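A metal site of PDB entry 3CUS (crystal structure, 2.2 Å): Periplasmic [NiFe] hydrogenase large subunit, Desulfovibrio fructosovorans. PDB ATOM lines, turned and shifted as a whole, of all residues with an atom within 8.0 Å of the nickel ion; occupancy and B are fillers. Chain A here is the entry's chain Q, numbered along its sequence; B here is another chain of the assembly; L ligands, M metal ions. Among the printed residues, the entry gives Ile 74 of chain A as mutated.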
ATOM      1  N   GLU A  25     -12.821 -28.067  -7.008  1.00  0.00           N
ATOM      2  CA  GLU A  25     -14.107 -27.420  -6.699  1.00  0.00           C
ATOM      3  C   GLU A  25     -14.466 -26.407  -7.794  1.00  0.00           C
ATOM      4  O   GLU A  25     -13.669 -25.498  -8.119  1.00  0.00           O
ATOM      5  CB  GLU A  25     -14.108 -26.728  -5.328  1.00  0.00           C
ATOM      6  CG  GLU A  25     -15.499 -26.288  -4.799  1.00  0.00           C
ATOM      7  CD  GLU A  25     -16.226 -25.260  -5.681  1.00  0.00           C
ATOM      8  OE1 GLU A  25     -15.589 -24.294  -6.141  1.00  0.00           O
ATOM      9  OE2 GLU A  25     -17.465 -25.436  -5.907  1.00  0.00           O
ATOM     10  N   GLN A  69     -19.525 -18.396   4.435  1.00  0.00           N
ATOM     11  CA  GLN A  69     -19.097 -19.779   4.550  1.00  0.00           C
ATOM     12  C   GLN A  69     -19.485 -20.505   3.263  1.00  0.00           C
ATOM     13  O   GLN A  69     -18.769 -21.376   2.814  1.00  0.00           O
ATOM     14  CB  GLN A  69     -19.647 -20.498   5.795  1.00  0.00           C
ATOM     15  CG  GLN A  69     -18.982 -21.862   5.954  1.00  0.00           C
ATOM     16  CD  GLN A  69     -19.217 -22.592   7.274  1.00  0.00           C
ATOM     17  OE1 GLN A  69     -18.490 -23.514   7.579  1.00  0.00           O
ATOM     18  NE2 GLN A  69     -20.262 -22.214   8.024  1.00  0.00           N
ATOM     19  N   ALA A  71     -19.276 -19.611   0.330  1.00  0.00           N
ATOM     20  CA  ALA A  71     -18.342 -19.444  -0.750  1.00  0.00           C
ATOM     21  C   ALA A  71     -17.829 -20.813  -1.184  1.00  0.00           C
ATOM     22  O   ALA A  71     -17.554 -21.028  -2.354  1.00  0.00           O
ATOM     23  CB  ALA A  71     -17.176 -18.550  -0.332  1.00  0.00           C
ATOM     24  N   CYS A  72     -17.649 -21.723  -0.207  1.00  0.00           N
ATOM     25  CA  CYS A  72     -17.058 -23.011  -0.491  1.00  0.00           C
ATOM     26  C   CYS A  72     -17.420 -24.072   0.538  1.00  0.00           C
ATOM     27  O   CYS A  72     -17.227 -23.878   1.745  1.00  0.00           O
ATOM     28  CB  CYS A  72     -15.532 -22.899  -0.572  1.00  0.00           C
ATOM     29  SG  CYS A  72     -14.714 -24.346  -1.334  1.00  0.00           S
ATOM     30  N   GLY A  73     -17.846 -25.227   0.045  1.00  0.00           N
ATOM     31  CA  GLY A  73     -18.106 -26.371   0.903  1.00  0.00           C
ATOM     32  C   GLY A  73     -16.991 -27.383   0.960  1.00  0.00           C
ATOM     33  O   GLY A  73     -17.057 -28.359   1.730  1.00  0.00           O
ATOM     34  N   ILE A  74     -15.953 -27.158   0.148  1.00  0.00           N
ATOM     35  CA  ILE A  74     -14.740 -27.963   0.248  1.00  0.00           C
ATOM     36  C   ILE A  74     -13.840 -27.376   1.316  1.00  0.00           C
ATOM     37  O   ILE A  74     -13.548 -28.064   2.310  1.00  0.00           O
ATOM     38  CB  ILE A  74     -13.989 -28.139  -1.085  1.00  0.00           C
ATOM     39  CG1 ILE A  74     -14.927 -28.737  -2.162  1.00  0.00           C
ATOM     40  CG2 ILE A  74     -12.761 -29.005  -0.846  1.00  0.00           C
ATOM     41  CD1 ILE A  74     -14.220 -29.558  -3.248  1.00  0.00           C
ATOM     42  N   CYS A  75     -13.443 -26.104   1.131  1.00  0.00           N
ATOM     43  CA  CYS A  75     -12.812 -25.339   2.235  1.00  0.00           C
ATOM     44  C   CYS A  75     -13.899 -24.743   3.127  1.00  0.00           C
ATOM     45  O   CYS A  75     -13.933 -23.542   3.372  1.00  0.00           O
ATOM     46  CB  CYS A  75     -11.836 -24.264   1.714  1.00  0.00           C
ATOM     47  SG  CYS A  75     -12.575 -22.945   0.759  1.00  0.00           S
ATOM     48  N   THR A  76     -14.837 -25.600   3.553  1.00  0.00           N
ATOM     49  CA  THR A  76     -15.868 -25.233   4.500  1.00  0.00           C
ATOM     50  C   THR A  76     -15.139 -24.679   5.744  1.00  0.00           C
ATOM     51  O   THR A  76     -13.947 -24.903   5.911  1.00  0.00           O
ATOM     52  CB  THR A  76     -16.785 -26.472   4.857  1.00  0.00           C
ATOM     53  OG1 THR A  76     -17.913 -26.049   5.634  1.00  0.00           O
ATOM     54  CG2 THR A  76     -16.023 -27.561   5.676  1.00  0.00           C
ATOM     55  N   VAL A  78     -13.497 -22.104   6.652  1.00  0.00           N
ATOM     56  CA  VAL A  78     -12.464 -21.068   6.561  1.00  0.00           C
ATOM     57  C   VAL A  78     -13.040 -19.658   6.327  1.00  0.00           C
ATOM     58  O   VAL A  78     -12.532 -18.689   6.903  1.00  0.00           O
ATOM     59  CB  VAL A  78     -11.327 -21.393   5.501  1.00  0.00           C
ATOM     60  CG1 VAL A  78     -10.797 -22.807   5.706  1.00  0.00           C
ATOM     61  CG2 VAL A  78     -11.804 -21.202   4.046  1.00  0.00           C
ATOM     62  N   HIS A  79     -14.083 -19.542   5.498  1.00  0.00           N
ATOM     63  CA  HIS A  79     -14.717 -18.251   5.268  1.00  0.00           C
ATOM     64  C   HIS A  79     -15.503 -17.769   6.477  1.00  0.00           C
ATOM     65  O   HIS A  79     -15.546 -16.559   6.763  1.00  0.00           O
ATOM     66  CB  HIS A  79     -15.618 -18.293   4.054  1.00  0.00           C
ATOM     67  CG  HIS A  79     -14.877 -18.465   2.771  1.00  0.00           C
ATOM     68  ND1 HIS A  79     -14.224 -17.420   2.160  1.00  0.00           N
ATOM     69  CD2 HIS A  79     -14.674 -19.554   1.996  1.00  0.00           C
ATOM     70  CE1 HIS A  79     -13.651 -17.854   1.059  1.00  0.00           C
ATOM     71  NE2 HIS A  79     -13.918 -19.133   0.921  1.00  0.00           N
ATOM     72  N   GLN A 110      -9.487 -28.991   9.491  1.00  0.00           N
ATOM     73  CA  GLN A 110      -9.851 -28.723   8.101  1.00  0.00           C
ATOM     74  C   GLN A 110      -8.690 -29.047   7.163  1.00  0.00           C
ATOM     75  O   GLN A 110      -8.911 -29.645   6.133  1.00  0.00           O
ATOM     76  CB  GLN A 110     -10.310 -27.279   7.918  1.00  0.00           C
ATOM     77  CG  GLN A 110     -10.585 -26.883   6.459  1.00  0.00           C
ATOM     78  CD  GLN A 110     -11.689 -27.716   5.797  1.00  0.00           C
ATOM     79  OE1 GLN A 110     -12.588 -28.229   6.473  1.00  0.00           O
ATOM     80  NE2 GLN A 110     -11.615 -27.861   4.486  1.00  0.00           N
ATOM     81  N   ASP A 114      -9.047 -31.708   4.234  1.00  0.00           N
ATOM     82  CA  ASP A 114      -8.962 -31.129   2.894  1.00  0.00           C
ATOM     83  C   ASP A 114      -7.782 -31.686   2.079  1.00  0.00           C
ATOM     84  O   ASP A 114      -7.943 -32.099   0.945  1.00  0.00           O
ATOM     85  CB  ASP A 114      -8.873 -29.596   3.037  1.00  0.00           C
ATOM     86  CG  ASP A 114      -9.338 -28.824   1.782  1.00  0.00           C
ATOM     87  OD1 ASP A 114      -9.183 -29.270   0.624  1.00  0.00           O
ATOM     88  OD2 ASP A 114      -9.835 -27.697   1.988  1.00  0.00           O
ATOM     89  N   ALA A 474      -5.918 -20.468   4.809  1.00  0.00           N
ATOM     90  CA  ALA A 474      -6.743 -21.621   4.532  1.00  0.00           C
ATOM     91  C   ALA A 474      -5.887 -22.679   3.834  1.00  0.00           C
ATOM     92  O   ALA A 474      -4.753 -22.394   3.434  1.00  0.00           O
ATOM     93  CB  ALA A 474      -7.907 -21.192   3.664  1.00  0.00           C
ATOM     94  N   PRO A 475      -6.422 -23.918   3.677  1.00  0.00           N
ATOM     95  CA  PRO A 475      -5.667 -24.993   3.013  1.00  0.00           C
ATOM     96  C   PRO A 475      -5.101 -24.574   1.655  1.00  0.00           C
ATOM     97  O   PRO A 475      -4.022 -25.029   1.298  1.00  0.00           O
ATOM     98  CB  PRO A 475      -6.719 -26.096   2.845  1.00  0.00           C
ATOM     99  CG  PRO A 475      -7.601 -25.914   4.070  1.00  0.00           C
ATOM    100  CD  PRO A 475      -7.746 -24.402   4.131  1.00  0.00           C
ATOM    101  N   ARG A 476      -5.801 -23.710   0.931  1.00  0.00           N
ATOM    102  CA  ARG A 476      -5.327 -23.262  -0.386  1.00  0.00           C
ATOM    103  C   ARG A 476      -4.522 -21.998  -0.336  1.00  0.00           C
ATOM    104  O   ARG A 476      -3.926 -21.611  -1.355  1.00  0.00           O
ATOM    105  CB  ARG A 476      -6.483 -23.138  -1.370  1.00  0.00           C
ATOM    106  CG  ARG A 476      -7.060 -24.500  -1.679  1.00  0.00           C
ATOM    107  CD  ARG A 476      -8.476 -24.460  -2.248  1.00  0.00           C
ATOM    108  NE  ARG A 476      -8.910 -25.836  -2.442  1.00  0.00           N
ATOM    109  CZ  ARG A 476      -9.328 -26.630  -1.457  1.00  0.00           C
ATOM    110  NH1 ARG A 476      -9.436 -26.154  -0.218  1.00  0.00           N
ATOM    111  NH2 ARG A 476      -9.637 -27.884  -1.711  1.00  0.00           N
ATOM    112  N   VAL A 497      -9.446 -14.254  -2.048  1.00  0.00           N
ATOM    113  CA  VAL A 497      -9.403 -15.658  -1.661  1.00  0.00           C
ATOM    114  C   VAL A 497      -8.197 -16.317  -2.303  1.00  0.00           C
ATOM    115  O   VAL A 497      -7.730 -15.833  -3.345  1.00  0.00           O
ATOM    116  CB  VAL A 497     -10.751 -16.357  -2.076  1.00  0.00           C
ATOM    117  CG1 VAL A 497     -10.921 -17.723  -1.384  1.00  0.00           C
ATOM    118  CG2 VAL A 497     -11.914 -15.452  -1.702  1.00  0.00           C
ATOM    119  N   PRO A 498      -7.620 -17.357  -1.636  1.00  0.00           N
ATOM    120  CA  PRO A 498      -6.424 -17.982  -2.209  1.00  0.00           C
ATOM    121  C   PRO A 498      -6.492 -18.315  -3.694  1.00  0.00           C
ATOM    122  O   PRO A 498      -5.584 -17.965  -4.440  1.00  0.00           O
ATOM    123  CB  PRO A 498      -6.209 -19.244  -1.353  1.00  0.00           C
ATOM    124  CG  PRO A 498      -7.287 -19.276  -0.310  1.00  0.00           C
ATOM    125  CD  PRO A 498      -7.931 -17.909  -0.311  1.00  0.00           C
ATOM    126  N   SER A 499      -7.556 -18.988  -4.131  1.00  0.00           N
ATOM    127  CA  SER A 499      -7.711 -19.274  -5.553  1.00  0.00           C
ATOM    128  C   SER A 499      -7.795 -18.025  -6.449  1.00  0.00           C
ATOM    129  O   SER A 499      -7.399 -18.080  -7.630  1.00  0.00           O
ATOM    130  CB  SER A 499      -8.898 -20.199  -5.812  1.00  0.00           C
ATOM    131  OG  SER A 499      -8.605 -21.535  -5.420  1.00  0.00           O
ATOM    132  N   ASP A 541      -4.570 -26.885  -6.319  1.00  0.00           N
ATOM    133  CA  ASP A 541      -5.783 -27.186  -5.539  1.00  0.00           C
ATOM    134  C   ASP A 541      -6.881 -26.133  -5.820  1.00  0.00           C
ATOM    135  O   ASP A 541      -7.305 -25.411  -4.920  1.00  0.00           O
ATOM    136  CB  ASP A 541      -5.418 -27.291  -4.044  1.00  0.00           C
ATOM    137  CG  ASP A 541      -6.494 -27.912  -3.193  1.00  0.00           C
ATOM    138  OD1 ASP A 541      -7.539 -28.305  -3.734  1.00  0.00           O
ATOM    139  OD2 ASP A 541      -6.274 -28.021  -1.968  1.00  0.00           O
ATOM    140  N   PRO A 542      -7.353 -26.036  -7.097  1.00  0.00           N
ATOM    141  CA  PRO A 542      -8.265 -24.960  -7.451  1.00  0.00           C
ATOM    142  C   PRO A 542      -9.631 -25.022  -6.771  1.00  0.00           C
ATOM    143  O   PRO A 542     -10.260 -26.082  -6.695  1.00  0.00           O
ATOM    144  CB  PRO A 542      -8.418 -25.099  -8.992  1.00  0.00           C
ATOM    145  CG  PRO A 542      -7.258 -25.864  -9.430  1.00  0.00           C
ATOM    146  CD  PRO A 542      -7.045 -26.873  -8.278  1.00  0.00           C
ATOM    147  N   CSO A 543     -10.102 -23.854  -6.347  1.00  0.00           N
ATOM    148  CA  CSO A 543     -11.439 -23.774  -5.788  1.00  0.00           C
ATOM    149  CB  CSO A 543     -11.289 -23.723  -4.270  1.00  0.00           C
ATOM    150  SG  CSO A 543     -12.799 -24.135  -3.440  1.00  0.00           S
ATOM    151  C   CSO A 543     -12.097 -22.524  -6.392  1.00  0.00           C
ATOM    152  O   CSO A 543     -11.751 -21.390  -6.035  1.00  0.00           O
ATOM    153  OD  CSO A 543     -14.203 -23.267  -4.066  1.00  0.00           O
ATOM    154  N   ILE A 544     -13.001 -22.743  -7.351  1.00  0.00           N
ATOM    155  CA  ILE A 544     -13.472 -21.643  -8.250  1.00  0.00           C
ATOM    156  C   ILE A 544     -14.608 -20.838  -7.594  1.00  0.00           C
ATOM    157  O   ILE A 544     -14.749 -19.631  -7.790  1.00  0.00           O
ATOM    158  CB  ILE A 544     -13.888 -22.183  -9.666  1.00  0.00           C
ATOM    159  CG1 ILE A 544     -12.808 -23.077 -10.274  1.00  0.00           C
ATOM    160  CG2 ILE A 544     -14.198 -21.028 -10.654  1.00  0.00           C
ATOM    161  CD1 ILE A 544     -11.373 -22.432 -10.345  1.00  0.00           C
ATOM    162  N   ALA A 545     -15.409 -21.544  -6.802  1.00  0.00           N
ATOM    163  CA  ALA A 545     -16.471 -20.899  -6.045  1.00  0.00           C
ATOM    164  C   ALA A 545     -15.804 -19.964  -5.056  1.00  0.00           C
ATOM    165  O   ALA A 545     -16.281 -18.852  -4.847  1.00  0.00           O
ATOM    166  CB  ALA A 545     -17.379 -21.961  -5.346  1.00  0.00           C
ATOM    167  N   CYS A 546     -14.708 -20.404  -4.460  1.00  0.00           N
ATOM    168  CA  CYS A 546     -13.859 -19.559  -3.595  1.00  0.00           C
ATOM    169  C   CYS A 546     -13.287 -18.366  -4.363  1.00  0.00           C
ATOM    170  O   CYS A 546     -13.414 -17.206  -3.945  1.00  0.00           O
ATOM    171  CB  CYS A 546     -12.713 -20.386  -3.046  1.00  0.00           C
ATOM    172  SG  CYS A 546     -12.937 -21.033  -1.410  1.00  0.00           S
ATOM    173  N   GLY A 547     -12.634 -18.627  -5.479  1.00  0.00           N
ATOM    174  CA  GLY A 547     -11.936 -17.564  -6.198  1.00  0.00           C
ATOM    175  C   GLY A 547     -12.849 -16.444  -6.738  1.00  0.00           C
ATOM    176  O   GLY A 547     -12.452 -15.299  -6.743  1.00  0.00           O
ATOM    177  N   CYS B  17     -21.566 -24.598  -4.071  1.00  0.00           N
ATOM    178  CA  CYS B  17     -20.338 -24.476  -3.342  1.00  0.00           C
ATOM    179  C   CYS B  17     -19.660 -25.828  -3.140  1.00  0.00           C
ATOM    180  O   CYS B  17     -18.591 -25.905  -2.523  1.00  0.00           O
ATOM    181  CB  CYS B  17     -20.596 -23.815  -1.976  1.00  0.00           C
ATOM    182  SG  CYS B  17     -21.240 -24.973  -0.674  1.00  0.00           S
HETATM  183 FE1  LIG L   1     -11.048 -21.900  -0.422  1.00  0.00          FE
HETATM  184  C1  LIG L   1      -9.973 -21.292  -1.866  1.00  0.00           C
HETATM  185  N1  LIG L   1      -9.322 -20.945  -2.753  1.00  0.00           N
HETATM  186  C2  LIG L   1      -9.575 -22.710   0.471  1.00  0.00           C
HETATM  187  N2  LIG L   1      -8.693 -23.178   1.066  1.00  0.00           N
HETATM  188  C3  LIG L   1     -10.713 -20.525   0.581  1.00  0.00           C
HETATM  189  O1  LIG L   1     -10.555 -19.637   1.273  1.00  0.00           O
HETATM  190 NI    NI M   1     -12.677 -23.588  -1.252  1.00  0.00          NI
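SG of Cys 75 is bound to the nickel ion (2.1 Å).
The nickel ion is bound by SG of Cys 72, 2.2 Å away.
SG of CSO 543 binds the nickel ion (2.3 Å).
SG of Cys 546 is bound to the nickel ion (2.6 Å).
The nearest printed residue that does not touch the nickel ion is Arg 476 (4.3 Å).
The guanidinium group (NH1) of Arg 476 lies close to a nitrogen (N2) of the ligand (3.3 Å).
An iron atom (FE1) of the ligand is bound by the side-chain sulfur (SG) of Cys 75 (2.2 Å).
The side-chain hydroxyl (OG) of Ser 499 lies within hydrogen-bond range of a nitrogen (N1) of the ligand (2.8 Å).
The side-chain sulfur (SG) of Cys 546 is bound to an iron atom (FE1) of the ligand (2.3 Å).
A nitrogen (N2) of the ligand is in hydrogen-bond range of the backbone NH (N) of Arg 476 (2.9 Å).
NE2 of His 79 is in hydrogen-bond range of O1 of the ligand (3.4 Å).
A nitrogen (N1) of the ligand sits at hydrogen-bond distance from the backbone NH of Ser 499, at 3.0 Å.
OE1 of Glu 25 lies within hydrogen-bond range of OD of CSO 543, 2.7 Å away.
The side-chain sulfur (SG) of Cys 72 sits close to the backbone NH (N) of Ile 74 (3.4 Å).
OD of CSO 543 lies within hydrogen-bond range of N of Ala 545 (3.5 Å).
NE2 of His 79 sits close to SG of Cys 546, at 3.2 Å.
OG of Ser 499 sits at hydrogen-bond distance from N of CSO 543 (2.9 Å).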
